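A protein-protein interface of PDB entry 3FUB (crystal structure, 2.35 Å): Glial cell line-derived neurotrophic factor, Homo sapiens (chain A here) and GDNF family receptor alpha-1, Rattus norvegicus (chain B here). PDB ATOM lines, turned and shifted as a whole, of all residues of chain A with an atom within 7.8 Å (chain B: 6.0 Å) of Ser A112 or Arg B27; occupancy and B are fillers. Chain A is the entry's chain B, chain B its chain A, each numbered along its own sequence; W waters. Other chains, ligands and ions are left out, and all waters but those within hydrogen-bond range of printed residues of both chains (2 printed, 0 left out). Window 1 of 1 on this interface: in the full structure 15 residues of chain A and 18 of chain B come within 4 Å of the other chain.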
ATOM      1  N   VAL A  50     -21.256  -7.790 -14.904  1.00  0.00           N
ATOM      2  CA  VAL A  50     -21.531  -6.367 -14.653  1.00  0.00           C
ATOM      3  C   VAL A  50     -22.970  -6.144 -14.167  1.00  0.00           C
ATOM      4  O   VAL A  50     -23.250  -5.192 -13.429  1.00  0.00           O
ATOM      5  CB  VAL A  50     -21.251  -5.494 -15.901  1.00  0.00           C
ATOM      6  CG1 VAL A  50     -21.778  -4.072 -15.702  1.00  0.00           C
ATOM      7  CG2 VAL A  50     -19.759  -5.461 -16.203  1.00  0.00           C
ATOM      8  N   GLU A  61     -21.191  -8.048 -20.428  1.00  0.00           N
ATOM      9  CA  GLU A  61     -19.779  -7.835 -20.129  1.00  0.00           C
ATOM     10  C   GLU A  61     -19.472  -8.138 -18.660  1.00  0.00           C
ATOM     11  O   GLU A  61     -20.386  -8.237 -17.840  1.00  0.00           O
ATOM     12  CB  GLU A  61     -19.326  -6.424 -20.535  1.00  0.00           C
ATOM     13  CG  GLU A  61     -19.205  -6.220 -22.053  1.00  0.00           C
ATOM     14  CD  GLU A  61     -17.928  -5.485 -22.483  1.00  0.00           C
ATOM     15  OE1 GLU A  61     -16.852  -5.712 -21.881  1.00  0.00           O
ATOM     16  OE2 GLU A  61     -17.997  -4.689 -23.446  1.00  0.00           O
ATOM     17  N   GLU A  62     -18.191  -8.305 -18.342  1.00  0.00           N
ATOM     18  CA  GLU A  62     -17.781  -8.871 -17.055  1.00  0.00           C
ATOM     19  C   GLU A  62     -16.656  -8.088 -16.373  1.00  0.00           C
ATOM     20  O   GLU A  62     -16.065  -7.188 -16.973  1.00  0.00           O
ATOM     21  CB  GLU A  62     -17.351 -10.330 -17.241  1.00  0.00           C
ATOM     22  CG  GLU A  62     -18.409 -11.232 -17.865  1.00  0.00           C
ATOM     23  CD  GLU A  62     -18.112 -12.713 -17.686  1.00  0.00           C
ATOM     24  OE1 GLU A  62     -17.048 -13.061 -17.118  1.00  0.00           O
ATOM     25  OE2 GLU A  62     -18.956 -13.533 -18.111  1.00  0.00           O
ATOM     26  N   LEU A  63     -16.368  -8.440 -15.118  1.00  0.00           N
ATOM     27  CA  LEU A  63     -15.297  -7.788 -14.357  1.00  0.00           C
ATOM     28  C   LEU A  63     -14.715  -8.632 -13.212  1.00  0.00           C
ATOM     29  O   LEU A  63     -15.243  -9.686 -12.857  1.00  0.00           O
ATOM     30  CB  LEU A  63     -15.754  -6.410 -13.842  1.00  0.00           C
ATOM     31  CG  LEU A  63     -16.692  -6.211 -12.640  1.00  0.00           C
ATOM     32  CD1 LEU A  63     -16.774  -4.734 -12.302  1.00  0.00           C
ATOM     33  CD2 LEU A  63     -18.090  -6.765 -12.872  1.00  0.00           C
ATOM     34  N   ASP A 109      -8.221   0.479 -11.629  1.00  0.00           N
ATOM     35  CA  ASP A 109      -8.387   1.217 -12.880  1.00  0.00           C
ATOM     36  C   ASP A 109      -9.838   1.196 -13.356  1.00  0.00           C
ATOM     37  O   ASP A 109     -10.581   0.255 -13.066  1.00  0.00           O
ATOM     38  CB  ASP A 109      -7.495   0.623 -13.970  1.00  0.00           C
ATOM     39  CG  ASP A 109      -6.021   0.838 -13.706  1.00  0.00           C
ATOM     40  OD1 ASP A 109      -5.615   1.973 -13.366  1.00  0.00           O
ATOM     41  OD2 ASP A 109      -5.259  -0.135 -13.856  1.00  0.00           O
ATOM     42  N   ASP A 110     -10.224   2.231 -14.103  1.00  0.00           N
ATOM     43  CA  ASP A 110     -11.566   2.327 -14.671  1.00  0.00           C
ATOM     44  C   ASP A 110     -11.885   1.091 -15.490  1.00  0.00           C
ATOM     45  O   ASP A 110     -11.009   0.546 -16.168  1.00  0.00           O
ATOM     46  CB  ASP A 110     -11.700   3.569 -15.550  1.00  0.00           C
ATOM     47  CG  ASP A 110     -11.527   4.864 -14.774  1.00  0.00           C
ATOM     48  OD1 ASP A 110     -11.375   4.816 -13.532  1.00  0.00           O
ATOM     49  OD2 ASP A 110     -11.543   5.939 -15.412  1.00  0.00           O
ATOM     50  N   LEU A 111     -13.132   0.639 -15.406  1.00  0.00           N
ATOM     51  CA  LEU A 111     -13.587  -0.487 -16.216  1.00  0.00           C
ATOM     52  C   LEU A 111     -14.651  -0.062 -17.229  1.00  0.00           C
ATOM     53  O   LEU A 111     -15.659   0.551 -16.867  1.00  0.00           O
ATOM     54  CB  LEU A 111     -14.081  -1.637 -15.337  1.00  0.00           C
ATOM     55  CG  LEU A 111     -14.329  -2.935 -16.108  1.00  0.00           C
ATOM     56  CD1 LEU A 111     -13.487  -4.064 -15.558  1.00  0.00           C
ATOM     57  CD2 LEU A 111     -15.809  -3.290 -16.118  1.00  0.00           C
ATOM     58  N   SER A 112     -14.394  -0.398 -18.495  1.00  0.00           N
ATOM     59  CA  SER A 112     -15.258  -0.044 -19.624  1.00  0.00           C
ATOM     60  C   SER A 112     -15.988  -1.258 -20.185  1.00  0.00           C
ATOM     61  O   SER A 112     -15.500  -2.385 -20.082  1.00  0.00           O
ATOM     62  CB  SER A 112     -14.436   0.604 -20.736  1.00  0.00           C
ATOM     63  OG  SER A 112     -14.035   1.916 -20.367  1.00  0.00           O
ATOM     64  N   PHE A 113     -17.155  -1.017 -20.783  1.00  0.00           N
ATOM     65  CA  PHE A 113     -17.958  -2.090 -21.367  1.00  0.00           C
ATOM     66  C   PHE A 113     -19.024  -1.583 -22.324  1.00  0.00           C
ATOM     67  O   PHE A 113     -19.528  -0.467 -22.177  1.00  0.00           O
ATOM     68  CB  PHE A 113     -18.600  -2.976 -20.280  1.00  0.00           C
ATOM     69  CG  PHE A 113     -19.596  -2.263 -19.399  1.00  0.00           C
ATOM     70  CD1 PHE A 113     -19.169  -1.507 -18.308  1.00  0.00           C
ATOM     71  CD2 PHE A 113     -20.965  -2.371 -19.643  1.00  0.00           C
ATOM     72  CE1 PHE A 113     -20.094  -0.846 -17.481  1.00  0.00           C
ATOM     73  CE2 PHE A 113     -21.896  -1.719 -18.825  1.00  0.00           C
ATOM     74  CZ  PHE A 113     -21.457  -0.955 -17.741  1.00  0.00           C
ATOM     75  N   LEU A 114     -19.357  -2.421 -23.302  1.00  0.00           N
ATOM     76  CA  LEU A 114     -20.423  -2.138 -24.256  1.00  0.00           C
ATOM     77  C   LEU A 114     -21.690  -2.860 -23.816  1.00  0.00           C
ATOM     78  O   LEU A 114     -21.698  -4.086 -23.685  1.00  0.00           O
ATOM     79  CB  LEU A 114     -20.016  -2.594 -25.660  1.00  0.00           C
ATOM     80  CG  LEU A 114     -20.935  -2.260 -26.833  1.00  0.00           C
ATOM     81  CD1 LEU A 114     -20.639  -0.879 -27.383  1.00  0.00           C
ATOM     82  CD2 LEU A 114     -20.749  -3.293 -27.916  1.00  0.00           C
ATOM     83  N   ASP A 115     -22.759  -2.099 -23.587  1.00  0.00           N
ATOM     84  CA  ASP A 115     -24.040  -2.695 -23.219  1.00  0.00           C
ATOM     85  C   ASP A 115     -24.720  -3.366 -24.420  1.00  0.00           C
ATOM     86  O   ASP A 115     -24.207  -3.308 -25.540  1.00  0.00           O
ATOM     87  CB  ASP A 115     -24.944  -1.674 -22.523  1.00  0.00           C
ATOM     88  CG  ASP A 115     -25.559  -0.666 -23.474  1.00  0.00           C
ATOM     89  OD1 ASP A 115     -25.333  -0.745 -24.699  1.00  0.00           O
ATOM     90  OD2 ASP A 115     -26.288   0.219 -22.982  1.00  0.00           O
ATOM     91  N   TYR A 120     -21.355   2.432 -24.887  1.00  0.00           N
ATOM     92  CA  TYR A 120     -20.271   2.205 -23.930  1.00  0.00           C
ATOM     93  C   TYR A 120     -20.565   2.889 -22.602  1.00  0.00           C
ATOM     94  O   TYR A 120     -21.272   3.891 -22.561  1.00  0.00           O
ATOM     95  CB  TYR A 120     -18.941   2.739 -24.468  1.00  0.00           C
ATOM     96  CG  TYR A 120     -18.254   1.867 -25.488  1.00  0.00           C
ATOM     97  CD1 TYR A 120     -17.581   0.706 -25.104  1.00  0.00           C
ATOM     98  CD2 TYR A 120     -18.251   2.218 -26.832  1.00  0.00           C
ATOM     99  CE1 TYR A 120     -16.936  -0.087 -26.042  1.00  0.00           C
ATOM    100  CE2 TYR A 120     -17.607   1.435 -27.781  1.00  0.00           C
ATOM    101  CZ  TYR A 120     -16.954   0.286 -27.380  1.00  0.00           C
ATOM    102  OH  TYR A 120     -16.319  -0.491 -28.317  1.00  0.00           O
ATOM    103  N   HIS A 121     -20.013   2.339 -21.523  1.00  0.00           N
ATOM    104  CA  HIS A 121     -20.087   2.951 -20.202  1.00  0.00           C
ATOM    105  C   HIS A 121     -18.748   2.763 -19.483  1.00  0.00           C
ATOM    106  O   HIS A 121     -17.999   1.831 -19.781  1.00  0.00           O
ATOM    107  CB  HIS A 121     -21.222   2.329 -19.371  1.00  0.00           C
ATOM    108  CG  HIS A 121     -22.588   2.515 -19.963  1.00  0.00           C
ATOM    109  ND1 HIS A 121     -23.408   3.569 -19.625  1.00  0.00           N
ATOM    110  CD2 HIS A 121     -23.281   1.775 -20.861  1.00  0.00           C
ATOM    111  CE1 HIS A 121     -24.541   3.476 -20.297  1.00  0.00           C
ATOM    112  NE2 HIS A 121     -24.490   2.395 -21.054  1.00  0.00           N
ATOM    113  N   ILE A 122     -18.439   3.654 -18.546  1.00  0.00           N
ATOM    114  CA  ILE A 122     -17.203   3.537 -17.770  1.00  0.00           C
ATOM    115  C   ILE A 122     -17.505   3.538 -16.274  1.00  0.00           C
ATOM    116  O   ILE A 122     -18.173   4.445 -15.767  1.00  0.00           O
ATOM    117  CB  ILE A 122     -16.181   4.656 -18.098  1.00  0.00           C
ATOM    118  CG1 ILE A 122     -16.116   4.914 -19.603  1.00  0.00           C
ATOM    119  CG2 ILE A 122     -14.798   4.282 -17.567  1.00  0.00           C
ATOM    120  CD1 ILE A 122     -15.519   6.255 -19.981  1.00  0.00           C
ATOM    121  N   LEU A 123     -17.014   2.508 -15.586  1.00  0.00           N
ATOM    122  CA  LEU A 123     -17.107   2.416 -14.131  1.00  0.00           C
ATOM    123  C   LEU A 123     -15.847   2.960 -13.448  1.00  0.00           C
ATOM    124  O   LEU A 123     -14.741   2.457 -13.667  1.00  0.00           O
ATOM    125  CB  LEU A 123     -17.369   0.968 -13.703  1.00  0.00           C
ATOM    126  CG  LEU A 123     -18.711   0.360 -14.117  1.00  0.00           C
ATOM    127  CD1 LEU A 123     -18.763  -1.100 -13.740  1.00  0.00           C
ATOM    128  CD2 LEU A 123     -19.884   1.119 -13.495  1.00  0.00           C
ATOM    129  N   ARG A 124     -16.029   3.994 -12.631  1.00  0.00           N
ATOM    130  CA  ARG A 124     -14.925   4.626 -11.907  1.00  0.00           C
ATOM    131  C   ARG A 124     -14.978   4.351 -10.402  1.00  0.00           C
ATOM    132  O   ARG A 124     -16.043   4.456  -9.783  1.00  0.00           O
ATOM    133  CB  ARG A 124     -14.922   6.137 -12.153  1.00  0.00           C
ATOM    134  CG  ARG A 124     -14.158   6.577 -13.389  1.00  0.00           C
ATOM    135  CD  ARG A 124     -14.180   8.095 -13.540  1.00  0.00           C
ATOM    136  NE  ARG A 124     -14.265   8.491 -14.946  1.00  0.00           N
ATOM    137  CZ  ARG A 124     -15.385   8.487 -15.668  1.00  0.00           C
ATOM    138  NH1 ARG A 124     -16.537   8.107 -15.124  1.00  0.00           N
ATOM    139  NH2 ARG A 124     -15.357   8.861 -16.941  1.00  0.00           N
ATOM    140  N   HIS A 126     -14.951   1.722  -8.762  1.00  0.00           N
ATOM    141  CA  HIS A 126     -15.912   0.666  -8.526  1.00  0.00           C
ATOM    142  C   HIS A 126     -15.273  -0.430  -7.679  1.00  0.00           C
ATOM    143  O   HIS A 126     -15.971  -1.147  -6.967  1.00  0.00           O
ATOM    144  CB  HIS A 126     -16.336   0.082  -9.873  1.00  0.00           C
ATOM    145  CG  HIS A 126     -15.197  -0.508 -10.643  1.00  0.00           C
ATOM    146  ND1 HIS A 126     -14.175   0.257 -11.162  1.00  0.00           N
ATOM    147  CD2 HIS A 126     -14.895  -1.792 -10.946  1.00  0.00           C
ATOM    148  CE1 HIS A 126     -13.302  -0.528 -11.767  1.00  0.00           C
ATOM    149  NE2 HIS A 126     -13.716  -1.777 -11.650  1.00  0.00           N
ATOM    150  N   ALA B  14     -13.987  -9.341 -25.129  1.00  0.00           N
ATOM    151  CA  ALA B  14     -14.182  -8.279 -24.133  1.00  0.00           C
ATOM    152  C   ALA B  14     -13.996  -8.767 -22.690  1.00  0.00           C
ATOM    153  O   ALA B  14     -13.470  -8.033 -21.853  1.00  0.00           O
ATOM    154  CB  ALA B  14     -15.541  -7.603 -24.313  1.00  0.00           C
ATOM    155  N   CYS B  17     -10.269  -9.227 -22.006  1.00  0.00           N
ATOM    156  CA  CYS B  17      -9.652  -7.907 -21.878  1.00  0.00           C
ATOM    157  C   CYS B  17      -9.929  -7.261 -20.516  1.00  0.00           C
ATOM    158  O   CYS B  17      -9.039  -6.655 -19.915  1.00  0.00           O
ATOM    159  CB  CYS B  17     -10.141  -6.999 -23.009  1.00  0.00           C
ATOM    160  SG  CYS B  17      -9.364  -5.362 -23.104  1.00  0.00           S
ATOM    161  N   ASN B  18     -11.162  -7.397 -20.030  1.00  0.00           N
ATOM    162  CA  ASN B  18     -11.540  -6.849 -18.728  1.00  0.00           C
ATOM    163  C   ASN B  18     -10.934  -7.613 -17.545  1.00  0.00           C
ATOM    164  O   ASN B  18     -10.745  -7.052 -16.462  1.00  0.00           O
ATOM    165  CB  ASN B  18     -13.064  -6.773 -18.598  1.00  0.00           C
ATOM    166  CG  ASN B  18     -13.643  -5.524 -19.227  1.00  0.00           C
ATOM    167  OD1 ASN B  18     -12.924  -4.699 -19.796  1.00  0.00           O
ATOM    168  ND2 ASN B  18     -14.955  -5.373 -19.123  1.00  0.00           N
ATOM    169  N   THR B  22      -3.662  -5.263 -17.852  1.00  0.00           N
ATOM    170  CA  THR B  22      -3.124  -4.425 -18.931  1.00  0.00           C
ATOM    171  C   THR B  22      -4.230  -3.955 -19.887  1.00  0.00           C
ATOM    172  O   THR B  22      -4.501  -2.756 -19.981  1.00  0.00           O
ATOM    173  CB  THR B  22      -1.987  -5.149 -19.711  1.00  0.00           C
ATOM    174  OG1 THR B  22      -0.980  -5.585 -18.791  1.00  0.00           O
ATOM    175  CG2 THR B  22      -1.342  -4.224 -20.731  1.00  0.00           C
ATOM    176  N   CYS B  23      -4.866  -4.907 -20.571  1.00  0.00           N
ATOM    177  CA  CYS B  23      -5.911  -4.622 -21.564  1.00  0.00           C
ATOM    178  C   CYS B  23      -7.020  -3.735 -21.008  1.00  0.00           C
ATOM    179  O   CYS B  23      -7.423  -2.761 -21.651  1.00  0.00           O
ATOM    180  CB  CYS B  23      -6.517  -5.920 -22.102  1.00  0.00           C
ATOM    181  SG  CYS B  23      -7.436  -5.732 -23.658  1.00  0.00           S
ATOM    182  N   LYS B  24      -7.496  -4.077 -19.810  1.00  0.00           N
ATOM    183  CA  LYS B  24      -8.560  -3.340 -19.137  1.00  0.00           C
ATOM    184  C   LYS B  24      -8.210  -1.864 -18.953  1.00  0.00           C
ATOM    185  O   LYS B  24      -9.030  -0.984 -19.245  1.00  0.00           O
ATOM    186  CB  LYS B  24      -8.905  -4.010 -17.796  1.00  0.00           C
ATOM    187  CG  LYS B  24      -8.984  -3.065 -16.601  1.00  0.00           C
ATOM    188  CD  LYS B  24      -9.760  -3.655 -15.455  1.00  0.00           C
ATOM    189  CE  LYS B  24      -9.050  -3.373 -14.151  1.00  0.00           C
ATOM    190  NZ  LYS B  24      -8.123  -4.484 -13.792  1.00  0.00           N
ATOM    191  N   LYS B  25      -6.989  -1.610 -18.479  1.00  0.00           N
ATOM    192  CA  LYS B  25      -6.508  -0.257 -18.229  1.00  0.00           C
ATOM    193  C   LYS B  25      -6.565   0.608 -19.483  1.00  0.00           C
ATOM    194  O   LYS B  25      -7.127   1.699 -19.455  1.00  0.00           O
ATOM    195  CB  LYS B  25      -5.083  -0.297 -17.655  1.00  0.00           C
ATOM    196  CG  LYS B  25      -4.396   1.063 -17.562  1.00  0.00           C
ATOM    197  CD  LYS B  25      -3.473   1.173 -16.347  1.00  0.00           C
ATOM    198  CE  LYS B  25      -2.126   0.495 -16.549  1.00  0.00           C
ATOM    199  NZ  LYS B  25      -1.253   0.659 -15.334  1.00  0.00           N
ATOM    200  N   TYR B  26      -5.994   0.111 -20.578  1.00  0.00           N
ATOM    201  CA  TYR B  26      -5.896   0.883 -21.819  1.00  0.00           C
ATOM    202  C   TYR B  26      -7.188   0.924 -22.632  1.00  0.00           C
ATOM    203  O   TYR B  26      -7.397   1.849 -23.418  1.00  0.00           O
ATOM    204  CB  TYR B  26      -4.704   0.417 -22.672  1.00  0.00           C
ATOM    205  CG  TYR B  26      -3.382   0.824 -22.064  1.00  0.00           C
ATOM    206  CD1 TYR B  26      -2.916   2.138 -22.175  1.00  0.00           C
ATOM    207  CD2 TYR B  26      -2.614  -0.089 -21.345  1.00  0.00           C
ATOM    208  CE1 TYR B  26      -1.716   2.527 -21.592  1.00  0.00           C
ATOM    209  CE2 TYR B  26      -1.408   0.290 -20.759  1.00  0.00           C
ATOM    210  CZ  TYR B  26      -0.966   1.597 -20.886  1.00  0.00           C
ATOM    211  OH  TYR B  26       0.225   1.974 -20.311  1.00  0.00           O
ATOM    212  N   ARG B  27      -8.051  -0.077 -22.440  1.00  0.00           N
ATOM    213  CA  ARG B  27      -9.384  -0.057 -23.048  1.00  0.00           C
ATOM    214  C   ARG B  27     -10.136   1.160 -22.508  1.00  0.00           C
ATOM    215  O   ARG B  27     -10.536   2.045 -23.267  1.00  0.00           O
ATOM    216  CB  ARG B  27     -10.142  -1.352 -22.748  1.00  0.00           C
ATOM    217  CG  ARG B  27     -11.385  -1.562 -23.609  1.00  0.00           C
ATOM    218  CD  ARG B  27     -12.329  -2.581 -22.987  1.00  0.00           C
ATOM    219  NE  ARG B  27     -13.480  -2.829 -23.852  1.00  0.00           N
ATOM    220  CZ  ARG B  27     -14.580  -3.488 -23.495  1.00  0.00           C
ATOM    221  NH1 ARG B  27     -14.712  -3.978 -22.266  1.00  0.00           N
ATOM    222  NH2 ARG B  27     -15.558  -3.654 -24.375  1.00  0.00           N
ATOM    223  N   SER B  28     -10.275   1.219 -21.185  1.00  0.00           N
ATOM    224  CA  SER B  28     -10.875   2.365 -20.500  1.00  0.00           C
ATOM    225  C   SER B  28     -10.202   3.701 -20.817  1.00  0.00           C
ATOM    226  O   SER B  28     -10.859   4.740 -20.827  1.00  0.00           O
ATOM    227  CB  SER B  28     -10.890   2.138 -18.989  1.00  0.00           C
ATOM    228  OG  SER B  28     -11.992   1.332 -18.612  1.00  0.00           O
ATOM    229  N   ALA B  29      -8.903   3.668 -21.088  1.00  0.00           N
ATOM    230  CA  ALA B  29      -8.166   4.877 -21.446  1.00  0.00           C
ATOM    231  C   ALA B  29      -8.510   5.412 -22.845  1.00  0.00           C
ATOM    232  O   ALA B  29      -8.209   6.572 -23.152  1.00  0.00           O
ATOM    233  CB  ALA B  29      -6.660   4.656 -21.301  1.00  0.00           C
ATOM    234  N   TYR B  30      -9.135   4.590 -23.686  1.00  0.00           N
ATOM    235  CA  TYR B  30      -9.586   5.087 -24.987  1.00  0.00           C
ATOM    236  C   TYR B  30     -11.074   5.361 -25.067  1.00  0.00           C
ATOM    237  O   TYR B  30     -11.504   6.321 -25.700  1.00  0.00           O
ATOM    238  CB  TYR B  30      -9.052   4.263 -26.175  1.00  0.00           C
ATOM    239  CG  TYR B  30      -9.806   3.025 -26.638  1.00  0.00           C
ATOM    240  CD1 TYR B  30      -9.318   1.753 -26.351  1.00  0.00           C
ATOM    241  CD2 TYR B  30     -10.946   3.124 -27.450  1.00  0.00           C
ATOM    242  CE1 TYR B  30      -9.969   0.604 -26.802  1.00  0.00           C
ATOM    243  CE2 TYR B  30     -11.604   1.975 -27.924  1.00  0.00           C
ATOM    244  CZ  TYR B  30     -11.109   0.718 -27.586  1.00  0.00           C
ATOM    245  OH  TYR B  30     -11.734  -0.431 -28.031  1.00  0.00           O
ATOM    246  N   ILE B  31     -11.846   4.522 -24.392  1.00  0.00           N
ATOM    247  CA  ILE B  31     -13.281   4.712 -24.255  1.00  0.00           C
ATOM    248  C   ILE B  31     -13.567   6.087 -23.652  1.00  0.00           C
ATOM    249  O   ILE B  31     -14.420   6.810 -24.163  1.00  0.00           O
ATOM    250  CB  ILE B  31     -13.910   3.546 -23.435  1.00  0.00           C
ATOM    251  CG1 ILE B  31     -13.803   2.230 -24.218  1.00  0.00           C
ATOM    252  CG2 ILE B  31     -15.359   3.822 -23.056  1.00  0.00           C
ATOM    253  CD1 ILE B  31     -14.365   2.285 -25.643  1.00  0.00           C
ATOM    254  N   THR B  32     -12.819   6.457 -22.608  1.00  0.00           N
ATOM    255  CA  THR B  32     -12.964   7.763 -21.946  1.00  0.00           C
ATOM    256  C   THR B  32     -12.997   8.949 -22.930  1.00  0.00           C
ATOM    257  O   THR B  32     -14.024   9.637 -23.015  1.00  0.00           O
ATOM    258  CB  THR B  32     -11.907   7.970 -20.826  1.00  0.00           C
ATOM    259  OG1 THR B  32     -12.044   6.935 -19.846  1.00  0.00           O
ATOM    260  CG2 THR B  32     -12.070   9.319 -20.134  1.00  0.00           C
ATOM    261  N   PHE B  55      -3.580   2.133 -27.266  1.00  0.00           N
ATOM    262  CA  PHE B  55      -4.214   0.851 -26.980  1.00  0.00           C
ATOM    263  C   PHE B  55      -3.524  -0.305 -27.712  1.00  0.00           C
ATOM    264  O   PHE B  55      -3.183  -1.315 -27.100  1.00  0.00           O
ATOM    265  CB  PHE B  55      -5.724   0.887 -27.278  1.00  0.00           C
ATOM    266  CG  PHE B  55      -6.423  -0.435 -27.052  1.00  0.00           C
ATOM    267  CD1 PHE B  55      -6.648  -0.907 -25.762  1.00  0.00           C
ATOM    268  CD2 PHE B  55      -6.842  -1.210 -28.132  1.00  0.00           C
ATOM    269  CE1 PHE B  55      -7.281  -2.125 -25.546  1.00  0.00           C
ATOM    270  CE2 PHE B  55      -7.480  -2.439 -27.930  1.00  0.00           C
ATOM    271  CZ  PHE B  55      -7.700  -2.894 -26.633  1.00  0.00           C
ATOM    272  N   VAL B  59      -0.925  -2.880 -25.490  1.00  0.00           N
ATOM    273  CA  VAL B  59      -1.578  -4.165 -25.209  1.00  0.00           C
ATOM    274  C   VAL B  59      -1.153  -5.228 -26.235  1.00  0.00           C
ATOM    275  O   VAL B  59      -1.227  -4.981 -27.437  1.00  0.00           O
ATOM    276  CB  VAL B  59      -3.126  -4.027 -25.184  1.00  0.00           C
ATOM    277  CG1 VAL B  59      -3.789  -5.328 -24.749  1.00  0.00           C
ATOM    278  CG2 VAL B  59      -3.552  -2.881 -24.276  1.00  0.00           C
ATOM    279  N   MET B  67     -10.442  -8.220 -29.722  1.00  0.00           N
ATOM    280  CA  MET B  67     -11.374  -7.095 -29.819  1.00  0.00           C
ATOM    281  C   MET B  67     -11.715  -6.687 -31.261  1.00  0.00           C
ATOM    282  O   MET B  67     -12.878  -6.434 -31.581  1.00  0.00           O
ATOM    283  CB  MET B  67     -10.797  -5.890 -29.065  1.00  0.00           C
ATOM    284  CG  MET B  67     -10.603  -6.127 -27.569  1.00  0.00           C
ATOM    285  SD  MET B  67     -12.169  -6.211 -26.682  1.00  0.00           S
ATOM    286  CE  MET B  67     -12.505  -4.472 -26.436  1.00  0.00           C
ATOM    287  N   ARG B  80     -21.103  -4.961 -32.645  1.00  0.00           N
ATOM    288  CA  ARG B  80     -20.142  -4.876 -31.543  1.00  0.00           C
ATOM    289  C   ARG B  80     -18.734  -4.657 -32.091  1.00  0.00           C
ATOM    290  O   ARG B  80     -18.042  -3.720 -31.684  1.00  0.00           O
ATOM    291  CB  ARG B  80     -20.175  -6.128 -30.656  1.00  0.00           C
ATOM    292  CG  ARG B  80     -18.965  -6.247 -29.717  1.00  0.00           C
ATOM    293  CD  ARG B  80     -19.132  -7.345 -28.685  1.00  0.00           C
ATOM    294  NE  ARG B  80     -19.996  -6.943 -27.577  1.00  0.00           N
ATOM    295  CZ  ARG B  80     -19.570  -6.365 -26.456  1.00  0.00           C
ATOM    296  NH1 ARG B  80     -18.280  -6.101 -26.282  1.00  0.00           N
ATOM    297  NH2 ARG B  80     -20.442  -6.043 -25.511  1.00  0.00           N
HETATM  298  O   HOH W   1     -22.887  -5.743 -27.009  1.00  0.00           O
HETATM  299  O   HOH W   2     -12.009  -2.146 -19.589  1.00  0.00           O
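Water W2 lies within hydrogen-bond range of the side-chain amide oxygen of Asn B18, the backbone NH of Ser A112 and the backbone carbonyl oxygen of Lys B24. Water W1 bridges the guanidinium group (NH2) of Arg B80 (2.9 Å) and the backbone carbonyl oxygen (O) of Asp A115 (3.1 Å).
The backbone carbonyl oxygen of Cys B17 sits at hydrogen-bond distance from the backbone NH of Lys B24. The guanidinium group of Arg B27 sits at hydrogen-bond distance from the side-chain amide oxygen of Asn B18 (3.1 Å). The backbone carbonyl oxygen (O) of Ser B28 is in hydrogen-bond range of the side-chain hydroxyl (OG1) of Thr B32, at 2.7 Å. OE2 of Glu A61 is in hydrogen-bond range of N of Leu A114 (2.6 Å). N of Leu A123 is in hydrogen-bond range of O of Leu A111 (2.7 Å). The side-chain sulfur of Cys B17 is disulfide-bonded to the side-chain sulfur of Cys B23 (2.0 Å).
Of the 17 printed residues of chain A, 10 touch a printed residue of chain B. Printed residues of chain A that touch a printed residue of chain B: Glu A61, Glu A62, Asp A109, Asp A110, Leu A111, Ser A112, Phe A113, Leu A114, Tyr A120 and Ile A122. Hydrophobic or aromatic side chains of chain A that line the printed part of chain B: Leu A111, Leu A114, Tyr A120 and Ile A122. Of the 18 printed residues of chain B, 9 touch a printed residue of chain A. Among the printed residues, Asp or Glu carboxylates within 4 Å of a Lys or Arg side-chain nitrogen of the other chain: Glu A61 with Arg B27 and Glu A61 with Arg B80.
The side-chain carboxylate (OE1) of Glu A61 sits at hydrogen-bond distance from the side-chain amide nitrogen (ND2) of Asn B18, 3.4 Å away. ND2 of Asn B18 is in hydrogen-bond range of O of Glu A62 (3.0 Å). The side-chain amide nitrogen (ND2) of Asn B18 is in hydrogen-bond range of the backbone carbonyl oxygen (O) of Ser A112. The guanidinium group of Arg B27 lies within salt-bridge range of the side-chain carboxylate of Glu A61 (2.8 Å). NH1 of Arg B27 lies within hydrogen-bond range of O of Ser A112. The backbone carbonyl oxygen (O) of Asp A110 sits at hydrogen-bond distance from the side-chain hydroxyl (OG) of Ser B28. The side-chain hydroxyl (OG) of Ser B28 sits close to the backbone NH (N) of Leu A111 (3.5 Å). The side-chain hydroxyl (OG) of Ser B28 sits at hydrogen-bond distance from the side-chain hydroxyl (OG) of Ser A112 (2.8 Å). NH1 of Arg B80 lies within salt-bridge range of OE2 of Glu A61, at 3.2 Å. NH2 of Arg B80 is in hydrogen-bond range of O of Leu A114 (3.0 Å).
Glu A61 touches Ala B14 (OE1 to CB, 3.3 Å). Asp A109 touches Lys B25 (OD2 to CD, 3.3 Å). Lys B24 touches Asp A110. Leu A111 touches Asn B18 (CD2 to ND2, 3.8 Å). Lys B24 touches Leu A111. CB of Ile B31 touches OG of Ser A112, 3.5 Å away. NH1 of Arg B27 touches CA of Phe A113 (3.9 Å). Ile B31 touches Tyr A120 (CD1 to CE1, 3.5 Å). CG2 of Ile B31 touches CG1 of Ile A122 (3.7 Å). CD1 of Ile A122 touches OG1 of Thr B32, at 3.5 Å.
Leu A63 touches none of the printed residues of chain B. Of the printed residues of chain B, Asp A110 touches Lys B24 and Ser B28. Of chain B, only Asn B18, Arg B27, Ser B28 and Ile B31 come within 4 Å of Ser A112. Of the printed residues of chain B, Phe A113 touches Arg B27 (3.9 Å). Of the printed residues of chain A, Arg B27 touches Glu A61 (2.8 Å), Ser A112 (2.8 Å) and Phe A113 (3.9 Å). Printed residues of chain A within 4 Å of Ser B28: Asp A110 (2.7 Å), Leu A111 (3.3 Å) and Ser A112 (2.8 Å). Ala B29 touches none of the printed residues of chain A.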
